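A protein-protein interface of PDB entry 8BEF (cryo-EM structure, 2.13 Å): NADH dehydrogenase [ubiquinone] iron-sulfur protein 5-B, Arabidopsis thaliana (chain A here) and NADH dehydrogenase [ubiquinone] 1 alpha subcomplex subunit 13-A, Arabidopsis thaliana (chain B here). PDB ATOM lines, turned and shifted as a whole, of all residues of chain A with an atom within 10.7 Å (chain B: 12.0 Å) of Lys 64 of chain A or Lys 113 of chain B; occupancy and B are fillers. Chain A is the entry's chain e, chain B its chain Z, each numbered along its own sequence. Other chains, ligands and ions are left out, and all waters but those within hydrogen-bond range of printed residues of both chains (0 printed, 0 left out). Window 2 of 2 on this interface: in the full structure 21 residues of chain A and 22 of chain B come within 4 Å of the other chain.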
ATOM      1  N   ARG A  53      21.815 -15.804   7.005  1.00  0.00           N
ATOM      2  CA  ARG A  53      22.792 -14.945   6.340  1.00  0.00           C
ATOM      3  C   ARG A  53      23.051 -13.672   7.144  1.00  0.00           C
ATOM      4  O   ARG A  53      24.204 -13.240   7.308  1.00  0.00           O
ATOM      5  CB  ARG A  53      22.296 -14.619   4.931  1.00  0.00           C
ATOM      6  CG  ARG A  53      22.847 -13.346   4.327  1.00  0.00           C
ATOM      7  CD  ARG A  53      22.258 -13.120   2.947  1.00  0.00           C
ATOM      8  NE  ARG A  53      22.915 -12.027   2.243  1.00  0.00           N
ATOM      9  CZ  ARG A  53      23.949 -12.183   1.428  1.00  0.00           C
ATOM     10  NH1 ARG A  53      24.475 -13.376   1.204  1.00  0.00           N
ATOM     11  NH2 ARG A  53      24.469 -11.116   0.830  1.00  0.00           N
ATOM     12  N   ARG A  56      25.251 -14.504   9.928  1.00  0.00           N
ATOM     13  CA  ARG A  56      26.635 -14.582   9.469  1.00  0.00           C
ATOM     14  C   ARG A  56      27.273 -13.199   9.426  1.00  0.00           C
ATOM     15  O   ARG A  56      28.433 -13.023   9.822  1.00  0.00           O
ATOM     16  CB  ARG A  56      26.702 -15.240   8.091  1.00  0.00           C
ATOM     17  CG  ARG A  56      27.199 -16.660   8.118  1.00  0.00           C
ATOM     18  CD  ARG A  56      27.209 -17.274   6.739  1.00  0.00           C
ATOM     19  NE  ARG A  56      26.478 -18.534   6.697  1.00  0.00           N
ATOM     20  CZ  ARG A  56      25.258 -18.673   6.204  1.00  0.00           C
ATOM     21  NH1 ARG A  56      24.602 -17.649   5.685  1.00  0.00           N
ATOM     22  NH2 ARG A  56      24.682 -19.871   6.226  1.00  0.00           N
ATOM     23  N   ILE A  57      26.526 -12.204   8.945  1.00  0.00           N
ATOM     24  CA  ILE A  57      27.053 -10.839   8.910  1.00  0.00           C
ATOM     25  C   ILE A  57      27.359 -10.352  10.324  1.00  0.00           C
ATOM     26  O   ILE A  57      28.427  -9.784  10.594  1.00  0.00           O
ATOM     27  CB  ILE A  57      26.073  -9.897   8.190  1.00  0.00           C
ATOM     28  CG1 ILE A  57      26.083 -10.164   6.686  1.00  0.00           C
ATOM     29  CG2 ILE A  57      26.424  -8.438   8.467  1.00  0.00           C
ATOM     30  CD1 ILE A  57      24.838  -9.685   5.988  1.00  0.00           C
ATOM     31  N   TYR A  58      26.425 -10.580  11.250  1.00  0.00           N
ATOM     32  CA  TYR A  58      26.639 -10.187  12.642  1.00  0.00           C
ATOM     33  C   TYR A  58      27.833 -10.920  13.250  1.00  0.00           C
ATOM     34  O   TYR A  58      28.605 -10.339  14.025  1.00  0.00           O
ATOM     35  CB  TYR A  58      25.369 -10.448  13.453  1.00  0.00           C
ATOM     36  CG  TYR A  58      25.583 -10.605  14.943  1.00  0.00           C
ATOM     37  CD1 TYR A  58      25.680  -9.497  15.773  1.00  0.00           C
ATOM     38  CD2 TYR A  58      25.680 -11.864  15.520  1.00  0.00           C
ATOM     39  CE1 TYR A  58      25.872  -9.639  17.132  1.00  0.00           C
ATOM     40  CE2 TYR A  58      25.873 -12.013  16.879  1.00  0.00           C
ATOM     41  CZ  TYR A  58      25.967 -10.903  17.678  1.00  0.00           C
ATOM     42  OH  TYR A  58      26.158 -11.055  19.032  1.00  0.00           O
ATOM     43  N   LYS A  59      27.991 -12.200  12.914  1.00  0.00           N
ATOM     44  CA  LYS A  59      29.112 -12.995  13.401  1.00  0.00           C
ATOM     45  C   LYS A  59      30.438 -12.409  12.940  1.00  0.00           C
ATOM     46  O   LYS A  59      31.378 -12.270  13.729  1.00  0.00           O
ATOM     47  CB  LYS A  59      28.972 -14.432  12.902  1.00  0.00           C
ATOM     48  CG  LYS A  59      29.767 -15.463  13.666  1.00  0.00           C
ATOM     49  CD  LYS A  59      29.091 -16.824  13.602  1.00  0.00           C
ATOM     50  CE  LYS A  59      27.577 -16.698  13.529  1.00  0.00           C
ATOM     51  NZ  LYS A  59      26.911 -18.007  13.751  1.00  0.00           N
ATOM     52  N   GLU A  60      30.536 -12.079  11.652  1.00  0.00           N
ATOM     53  CA  GLU A  60      31.771 -11.500  11.137  1.00  0.00           C
ATOM     54  C   GLU A  60      32.044 -10.141  11.771  1.00  0.00           C
ATOM     55  O   GLU A  60      33.200  -9.791  12.041  1.00  0.00           O
ATOM     56  CB  GLU A  60      31.706 -11.393   9.615  1.00  0.00           C
ATOM     57  CG  GLU A  60      32.969 -10.834   8.987  1.00  0.00           C
ATOM     58  CD  GLU A  60      34.048 -11.886   8.835  1.00  0.00           C
ATOM     59  OE1 GLU A  60      33.712 -13.047   8.522  1.00  0.00           O
ATOM     60  OE2 GLU A  60      35.235 -11.551   9.030  1.00  0.00           O
ATOM     61  N   GLU A  61      30.987  -9.366  12.030  1.00  0.00           N
ATOM     62  CA  GLU A  61      31.172  -8.100  12.731  1.00  0.00           C
ATOM     63  C   GLU A  61      31.729  -8.321  14.132  1.00  0.00           C
ATOM     64  O   GLU A  61      32.616  -7.585  14.579  1.00  0.00           O
ATOM     65  CB  GLU A  61      29.855  -7.330  12.798  1.00  0.00           C
ATOM     66  CG  GLU A  61      30.034  -5.842  13.008  1.00  0.00           C
ATOM     67  CD  GLU A  61      28.760  -5.157  13.460  1.00  0.00           C
ATOM     68  OE1 GLU A  61      27.837  -5.857  13.926  1.00  0.00           O
ATOM     69  OE2 GLU A  61      28.682  -3.915  13.351  1.00  0.00           O
ATOM     70  N   GLN A  62      31.222  -9.331  14.841  1.00  0.00           N
ATOM     71  CA  GLN A  62      31.723  -9.603  16.185  1.00  0.00           C
ATOM     72  C   GLN A  62      33.139 -10.168  16.152  1.00  0.00           C
ATOM     73  O   GLN A  62      33.897  -9.999  17.112  1.00  0.00           O
ATOM     74  CB  GLN A  62      30.785 -10.564  16.915  1.00  0.00           C
ATOM     75  CG  GLN A  62      30.398 -10.135  18.325  1.00  0.00           C
ATOM     76  CD  GLN A  62      29.718  -8.776  18.372  1.00  0.00           C
ATOM     77  OE1 GLN A  62      29.138  -8.320  17.387  1.00  0.00           O
ATOM     78  NE2 GLN A  62      29.787  -8.123  19.526  1.00  0.00           N
ATOM     79  N   ARG A  63      33.502 -10.851  15.066  1.00  0.00           N
ATOM     80  CA  ARG A  63      34.847 -11.402  14.947  1.00  0.00           C
ATOM     81  C   ARG A  63      35.872 -10.311  14.651  1.00  0.00           C
ATOM     82  O   ARG A  63      36.991 -10.347  15.177  1.00  0.00           O
ATOM     83  CB  ARG A  63      34.877 -12.476  13.861  1.00  0.00           C
ATOM     84  CG  ARG A  63      36.154 -13.273  13.814  1.00  0.00           C
ATOM     85  CD  ARG A  63      36.283 -14.030  12.504  1.00  0.00           C
ATOM     86  NE  ARG A  63      36.449 -13.138  11.365  1.00  0.00           N
ATOM     87  CZ  ARG A  63      37.602 -12.592  11.003  1.00  0.00           C
ATOM     88  NH1 ARG A  63      38.714 -12.811  11.686  1.00  0.00           N
ATOM     89  NH2 ARG A  63      37.640 -11.808   9.930  1.00  0.00           N
ATOM     90  N   LYS A  64      35.512  -9.331  13.819  1.00  0.00           N
ATOM     91  CA  LYS A  64      36.429  -8.256  13.449  1.00  0.00           C
ATOM     92  C   LYS A  64      36.361  -7.064  14.396  1.00  0.00           C
ATOM     93  O   LYS A  64      36.644  -5.932  13.979  1.00  0.00           O
ATOM     94  CB  LYS A  64      36.162  -7.798  12.014  1.00  0.00           C
ATOM     95  CG  LYS A  64      36.488  -8.819  10.950  1.00  0.00           C
ATOM     96  CD  LYS A  64      36.277  -8.232   9.564  1.00  0.00           C
ATOM     97  CE  LYS A  64      37.274  -8.795   8.565  1.00  0.00           C
ATOM     98  NZ  LYS A  64      37.475  -7.880   7.409  1.00  0.00           N
ATOM     99  N   LEU A  65      35.994  -7.277  15.655  1.00  0.00           N
ATOM    100  CA  LEU A  65      35.893  -6.180  16.610  1.00  0.00           C
ATOM    101  C   LEU A  65      36.420  -6.582  17.984  1.00  0.00           C
ATOM    102  O   LEU A  65      35.995  -7.584  18.554  1.00  0.00           O
ATOM    103  CB  LEU A  65      34.444  -5.705  16.727  1.00  0.00           C
ATOM    104  CG  LEU A  65      34.155  -4.680  17.823  1.00  0.00           C
ATOM    105  CD1 LEU A  65      34.920  -3.388  17.574  1.00  0.00           C
ATOM    106  CD2 LEU A  65      32.661  -4.412  17.934  1.00  0.00           C
ATOM    107  N   TYR B 104      22.809   0.328   3.646  1.00  0.00           N
ATOM    108  CA  TYR B 104      23.015  -0.976   4.267  1.00  0.00           C
ATOM    109  C   TYR B 104      23.857  -1.887   3.381  1.00  0.00           C
ATOM    110  O   TYR B 104      24.646  -2.694   3.881  1.00  0.00           O
ATOM    111  CB  TYR B 104      21.671  -1.634   4.587  1.00  0.00           C
ATOM    112  CG  TYR B 104      21.805  -3.079   5.005  1.00  0.00           C
ATOM    113  CD1 TYR B 104      22.182  -3.414   6.297  1.00  0.00           C
ATOM    114  CD2 TYR B 104      21.570  -4.107   4.104  1.00  0.00           C
ATOM    115  CE1 TYR B 104      22.314  -4.730   6.680  1.00  0.00           C
ATOM    116  CE2 TYR B 104      21.700  -5.424   4.478  1.00  0.00           C
ATOM    117  CZ  TYR B 104      22.072  -5.732   5.765  1.00  0.00           C
ATOM    118  OH  TYR B 104      22.202  -7.047   6.139  1.00  0.00           O
ATOM    119  N   LEU B 105      23.695  -1.782   2.063  1.00  0.00           N
ATOM    120  CA  LEU B 105      24.513  -2.584   1.160  1.00  0.00           C
ATOM    121  C   LEU B 105      25.979  -2.180   1.232  1.00  0.00           C
ATOM    122  O   LEU B 105      26.863  -3.042   1.211  1.00  0.00           O
ATOM    123  CB  LEU B 105      23.986  -2.476  -0.269  1.00  0.00           C
ATOM    124  CG  LEU B 105      23.228  -3.713  -0.747  1.00  0.00           C
ATOM    125  CD1 LEU B 105      22.246  -4.176   0.315  1.00  0.00           C
ATOM    126  CD2 LEU B 105      22.507  -3.426  -2.049  1.00  0.00           C
ATOM    127  N   GLU B 106      26.259  -0.878   1.317  1.00  0.00           N
ATOM    128  CA  GLU B 106      27.643  -0.450   1.518  1.00  0.00           C
ATOM    129  C   GLU B 106      28.191  -0.971   2.843  1.00  0.00           C
ATOM    130  O   GLU B 106      29.339  -1.438   2.915  1.00  0.00           O
ATOM    131  CB  GLU B 106      27.745   1.073   1.459  1.00  0.00           C
ATOM    132  CG  GLU B 106      27.125   1.694   0.228  1.00  0.00           C
ATOM    133  CD  GLU B 106      26.549   3.068   0.504  1.00  0.00           C
ATOM    134  OE1 GLU B 106      26.665   3.542   1.654  1.00  0.00           O
ATOM    135  OE2 GLU B 106      25.985   3.676  -0.429  1.00  0.00           O
ATOM    136  N   TYR B 107      27.377  -0.911   3.898  1.00  0.00           N
ATOM    137  CA  TYR B 107      27.783  -1.454   5.192  1.00  0.00           C
ATOM    138  C   TYR B 107      28.135  -2.936   5.086  1.00  0.00           C
ATOM    139  O   TYR B 107      29.171  -3.380   5.596  1.00  0.00           O
ATOM    140  CB  TYR B 107      26.662  -1.228   6.207  1.00  0.00           C
ATOM    141  CG  TYR B 107      26.880  -1.864   7.559  1.00  0.00           C
ATOM    142  CD1 TYR B 107      26.487  -3.175   7.805  1.00  0.00           C
ATOM    143  CD2 TYR B 107      27.467  -1.154   8.593  1.00  0.00           C
ATOM    144  CE1 TYR B 107      26.682  -3.758   9.040  1.00  0.00           C
ATOM    145  CE2 TYR B 107      27.664  -1.728   9.831  1.00  0.00           C
ATOM    146  CZ  TYR B 107      27.270  -3.031  10.047  1.00  0.00           C
ATOM    147  OH  TYR B 107      27.465  -3.605  11.281  1.00  0.00           O
ATOM    148  N   GLU B 108      27.278  -3.717   4.428  1.00  0.00           N
ATOM    149  CA  GLU B 108      27.515  -5.152   4.305  1.00  0.00           C
ATOM    150  C   GLU B 108      28.738  -5.439   3.442  1.00  0.00           C
ATOM    151  O   GLU B 108      29.495  -6.379   3.717  1.00  0.00           O
ATOM    152  CB  GLU B 108      26.275  -5.839   3.733  1.00  0.00           C
ATOM    153  CG  GLU B 108      26.502  -7.260   3.249  1.00  0.00           C
ATOM    154  CD  GLU B 108      25.214  -7.951   2.844  1.00  0.00           C
ATOM    155  OE1 GLU B 108      25.221  -8.691   1.841  1.00  0.00           O
ATOM    156  OE2 GLU B 108      24.190  -7.748   3.529  1.00  0.00           O
ATOM    157  N   ALA B 109      28.944  -4.645   2.390  1.00  0.00           N
ATOM    158  CA  ALA B 109      30.143  -4.791   1.574  1.00  0.00           C
ATOM    159  C   ALA B 109      31.397  -4.575   2.408  1.00  0.00           C
ATOM    160  O   ALA B 109      32.376  -5.316   2.274  1.00  0.00           O
ATOM    161  CB  ALA B 109      30.101  -3.815   0.403  1.00  0.00           C
ATOM    162  N   ASP B 110      31.382  -3.564   3.278  1.00  0.00           N
ATOM    163  CA  ASP B 110      32.535  -3.326   4.142  1.00  0.00           C
ATOM    164  C   ASP B 110      32.734  -4.474   5.127  1.00  0.00           C
ATOM    165  O   ASP B 110      33.839  -5.016   5.244  1.00  0.00           O
ATOM    166  CB  ASP B 110      32.368  -2.003   4.888  1.00  0.00           C
ATOM    167  CG  ASP B 110      33.526  -1.708   5.819  1.00  0.00           C
ATOM    168  OD1 ASP B 110      34.655  -2.162   5.536  1.00  0.00           O
ATOM    169  OD2 ASP B 110      33.306  -1.020   6.838  1.00  0.00           O
ATOM    170  N   VAL B 111      31.670  -4.864   5.836  1.00  0.00           N
ATOM    171  CA  VAL B 111      31.803  -5.859   6.900  1.00  0.00           C
ATOM    172  C   VAL B 111      32.242  -7.202   6.332  1.00  0.00           C
ATOM    173  O   VAL B 111      33.118  -7.873   6.892  1.00  0.00           O
ATOM    174  CB  VAL B 111      30.484  -5.983   7.688  1.00  0.00           C
ATOM    175  CG1 VAL B 111      30.361  -7.368   8.307  1.00  0.00           C
ATOM    176  CG2 VAL B 111      30.401  -4.919   8.757  1.00  0.00           C
ATOM    177  N   MET B 112      31.649  -7.614   5.217  1.00  0.00           N
ATOM    178  CA  MET B 112      31.951  -8.903   4.614  1.00  0.00           C
ATOM    179  C   MET B 112      33.126  -8.854   3.652  1.00  0.00           C
ATOM    180  O   MET B 112      33.406  -9.859   2.991  1.00  0.00           O
ATOM    181  CB  MET B 112      30.717  -9.460   3.902  1.00  0.00           C
ATOM    182  CG  MET B 112      29.517  -9.627   4.813  1.00  0.00           C
ATOM    183  SD  MET B 112      29.966 -10.461   6.346  1.00  0.00           S
ATOM    184  CE  MET B 112      29.519 -12.149   5.950  1.00  0.00           C
ATOM    185  N   LYS B 113      33.809  -7.718   3.544  1.00  0.00           N
ATOM    186  CA  LYS B 113      35.089  -7.698   2.855  1.00  0.00           C
ATOM    187  C   LYS B 113      36.026  -8.691   3.528  1.00  0.00           C
ATOM    188  O   LYS B 113      36.057  -8.790   4.759  1.00  0.00           O
ATOM    189  CB  LYS B 113      35.684  -6.291   2.875  1.00  0.00           C
ATOM    190  CG  LYS B 113      36.983  -6.148   2.100  1.00  0.00           C
ATOM    191  CD  LYS B 113      37.459  -4.708   2.084  1.00  0.00           C
ATOM    192  CE  LYS B 113      38.883  -4.604   1.566  1.00  0.00           C
ATOM    193  NZ  LYS B 113      39.415  -3.219   1.681  1.00  0.00           N
ATOM    194  N   ASP B 114      36.750  -9.462   2.712  1.00  0.00           N
ATOM    195  CA  ASP B 114      37.670 -10.507   3.157  1.00  0.00           C
ATOM    196  C   ASP B 114      36.954 -11.740   3.694  1.00  0.00           C
ATOM    197  O   ASP B 114      37.553 -12.534   4.424  1.00  0.00           O
ATOM    198  CB  ASP B 114      38.668  -9.986   4.201  1.00  0.00           C
ATOM    199  CG  ASP B 114      39.947  -9.470   3.577  1.00  0.00           C
ATOM    200  OD1 ASP B 114      40.386 -10.042   2.557  1.00  0.00           O
ATOM    201  OD2 ASP B 114      40.512  -8.490   4.105  1.00  0.00           O
ATOM    202  N   VAL B 115      35.684 -11.924   3.351  1.00  0.00           N
ATOM    203  CA  VAL B 115      34.978 -13.180   3.572  1.00  0.00           C
ATOM    204  C   VAL B 115      34.751 -13.817   2.203  1.00  0.00           C
ATOM    205  O   VAL B 115      33.892 -13.351   1.439  1.00  0.00           O
ATOM    206  CB  VAL B 115      33.655 -12.982   4.321  1.00  0.00           C
ATOM    207  CG1 VAL B 115      33.206 -14.293   4.933  1.00  0.00           C
ATOM    208  CG2 VAL B 115      33.803 -11.923   5.390  1.00  0.00           C
ATOM    209  N   PRO B 116      35.494 -14.861   1.846  1.00  0.00           N
ATOM    210  CA  PRO B 116      35.397 -15.406   0.489  1.00  0.00           C
ATOM    211  C   PRO B 116      34.043 -16.045   0.226  1.00  0.00           C
ATOM    212  O   PRO B 116      33.397 -16.588   1.125  1.00  0.00           O
ATOM    213  CB  PRO B 116      36.519 -16.449   0.447  1.00  0.00           C
ATOM    214  CG  PRO B 116      36.676 -16.872   1.870  1.00  0.00           C
ATOM    215  CD  PRO B 116      36.396 -15.651   2.700  1.00  0.00           C
ATOM    216  N   GLY B 117      33.621 -15.973  -1.036  1.00  0.00           N
ATOM    217  CA  GLY B 117      32.380 -16.573  -1.470  1.00  0.00           C
ATOM    218  C   GLY B 117      31.141 -15.743  -1.228  1.00  0.00           C
ATOM    219  O   GLY B 117      30.052 -16.151  -1.649  1.00  0.00           O
ATOM    220  N   TRP B 118      31.264 -14.594  -0.571  1.00  0.00           N
ATOM    221  CA  TRP B 118      30.107 -13.761  -0.297  1.00  0.00           C
ATOM    222  C   TRP B 118      29.601 -13.089  -1.571  1.00  0.00           C
ATOM    223  O   TRP B 118      30.317 -12.942  -2.564  1.00  0.00           O
ATOM    224  CB  TRP B 118      30.442 -12.702   0.754  1.00  0.00           C
ATOM    225  CG  TRP B 118      29.259 -12.274   1.552  1.00  0.00           C
ATOM    226  CD1 TRP B 118      28.648 -11.056   1.522  1.00  0.00           C
ATOM    227  CD2 TRP B 118      28.525 -13.069   2.491  1.00  0.00           C
ATOM    228  NE1 TRP B 118      27.581 -11.038   2.388  1.00  0.00           N
ATOM    229  CE2 TRP B 118      27.484 -12.262   2.998  1.00  0.00           C
ATOM    230  CE3 TRP B 118      28.647 -14.380   2.955  1.00  0.00           C
ATOM    231  CZ2 TRP B 118      26.573 -12.726   3.943  1.00  0.00           C
ATOM    232  CZ3 TRP B 118      27.741 -14.839   3.895  1.00  0.00           C
ATOM    233  CH2 TRP B 118      26.718 -14.013   4.378  1.00  0.00           C
ATOM    234  N   LYS B 119      28.329 -12.695  -1.529  1.00  0.00           N
ATOM    235  CA  LYS B 119      27.705 -11.883  -2.567  1.00  0.00           C
ATOM    236  C   LYS B 119      26.833 -10.851  -1.876  1.00  0.00           C
ATOM    237  O   LYS B 119      25.866 -11.210  -1.198  1.00  0.00           O
ATOM    238  CB  LYS B 119      26.871 -12.732  -3.529  1.00  0.00           C
ATOM    239  CG  LYS B 119      27.681 -13.521  -4.535  1.00  0.00           C
ATOM    240  CD  LYS B 119      26.917 -14.739  -5.022  1.00  0.00           C
ATOM    241  CE  LYS B 119      27.649 -15.427  -6.160  1.00  0.00           C
ATOM    242  NZ  LYS B 119      27.620 -14.607  -7.402  1.00  0.00           N
ATOM    243  N   VAL B 120      27.168  -9.573  -2.051  1.00  0.00           N
ATOM    244  CA  VAL B 120      26.524  -8.518  -1.279  1.00  0.00           C
ATOM    245  C   VAL B 120      25.081  -8.356  -1.734  1.00  0.00           C
ATOM    246  O   VAL B 120      24.801  -8.213  -2.932  1.00  0.00           O
ATOM    247  CB  VAL B 120      27.311  -7.206  -1.410  1.00  0.00           C
ATOM    248  CG1 VAL B 120      26.483  -6.031  -0.913  1.00  0.00           C
ATOM    249  CG2 VAL B 120      28.620  -7.306  -0.643  1.00  0.00           C
ATOM    250  N   GLY B 121      24.158  -8.382  -0.778  1.00  0.00           N
ATOM    251  CA  GLY B 121      22.742  -8.256  -1.088  1.00  0.00           C
ATOM    252  C   GLY B 121      22.195  -9.383  -1.938  1.00  0.00           C
ATOM    253  O   GLY B 121      21.402  -9.136  -2.854  1.00  0.00           O
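Printed residues of chain B within 4 Å of Lys 64 of chain A: Lys 113. Of chain A, only Lys 64 comes within 4 Å of Lys 113 of chain B. Printed residues of chain B within 4 Å of Glu 60 of chain A: Val 111, Met 112 and Val 115. No residue of chain B comes within 4 Å of Leu 65 of chain A. No residue of chain A comes within 4 Å of Ala 109 of chain B. Met 112 of chain B touches just these residues of chain A: Ile 57 and Glu 60. Val 115 of chain B touches just one residue of chain A: Glu 60 (3.3 Å). Of the printed residues of chain A, Tyr 104 of chain B touches Ile 57 (3.7 Å). Printed residues of chain A within 4 Å of Gly 121 of chain B: Arg 53 (3.2 Å). Printed residues of chain A within 4 Å of Val 111 of chain B: Ile 57 (3.8 Å) and Glu 60 (3.6 Å). Printed residues of chain B within 4 Å of Ile 57 of chain A: Tyr 104 (3.7 Å), Glu 108 (3.2 Å), Val 111 (3.8 Å), Met 112 (3.9 Å) and Trp 118 (3.8 Å). Of the printed residues of chain A, Val 120 of chain B touches Arg 53. The nearest printed residue of chain B that does not touch Lys 64 of chain A is Asp 114 of chain B (4.02 Å).
Among the printed residues, pairs that only touch across the chains: Ile 57 of chain A with Glu 108 of chain B (3.2 Å), Glu 60 of chain A with Val 115 of chain B (3.3 Å), Glu 60 of chain A with Val 111 of chain B (3.6 Å), Ile 57 of chain A with Tyr 104 of chain B (3.7 Å), Arg 56 of chain A with Trp 118 of chain B (3.8 Å), Ile 57 of chain A with Trp 118 of chain B (3.8 Å), Arg 53 of chain A with Val 120 of chain B (3.8 Å), Glu 60 of chain A with Met 112 of chain B (3.8 Å), Ile 57 of chain A with Val 111 of chain B (3.8 Å) and Ile 57 of chain A with Met 112 of chain B (3.9 Å).
OH of Tyr 107 of chain B lies within hydrogen-bond range of OE2 of Glu 61 of chain A, 2.4 Å away. NH2 of Arg 53 of chain A lies within salt-bridge range of OE1 of Glu 108 of chain B, 2.7 Å away. NZ of Lys 64 of chain A sits at hydrogen-bond distance from O of Lys 113 of chain B (3.1 Å). O of Lys 119 of chain B sits at hydrogen-bond distance from NH2 of Arg 53 of chain A, at 2.5 Å. NH2 of Arg 53 of chain A sits close to NE1 of Trp 118 of chain B (3.5 Å). The guanidinium group (NH2) of Arg 53 of chain A sits close to the backbone NH (N) of Gly 121 of chain B, at 3.2 Å.
Hydrophobic or aromatic side chains of chain A that line the printed part of chain B: Ile 57. Hydrophobic or aromatic side chains of chain B within 4 Å of the printed part of chain A: Tyr 104, Tyr 107, Val 111, Met 112, Val 115 and Trp 118. Among the printed residues, 16 pairs touch across the chains. Among the printed residues, Asp or Glu carboxylates within 4 Å of a Lys or Arg side-chain nitrogen of the other chain: Arg 53 of chain A with Glu 108 of chain B.
The side-chain hydroxyl (OH) of Tyr 104 of chain B lies within hydrogen-bond range of the side-chain carboxylate (OE2) of Glu 108 of chain B (3.4 Å). The indole nitrogen (NE1) of Trp 118 of chain B is in hydrogen-bond range of the side-chain carboxylate (OE1) of Glu 108 of chain B (3.4 Å). The backbone NH (N) of Gly 121 of chain B is in hydrogen-bond range of the side-chain carboxylate (OE1) of Glu 108 of chain B (2.8 Å). The guanidinium group of Arg 63 of chain A lies within salt-bridge range of the side-chain carboxylate of Glu 60 of chain A.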
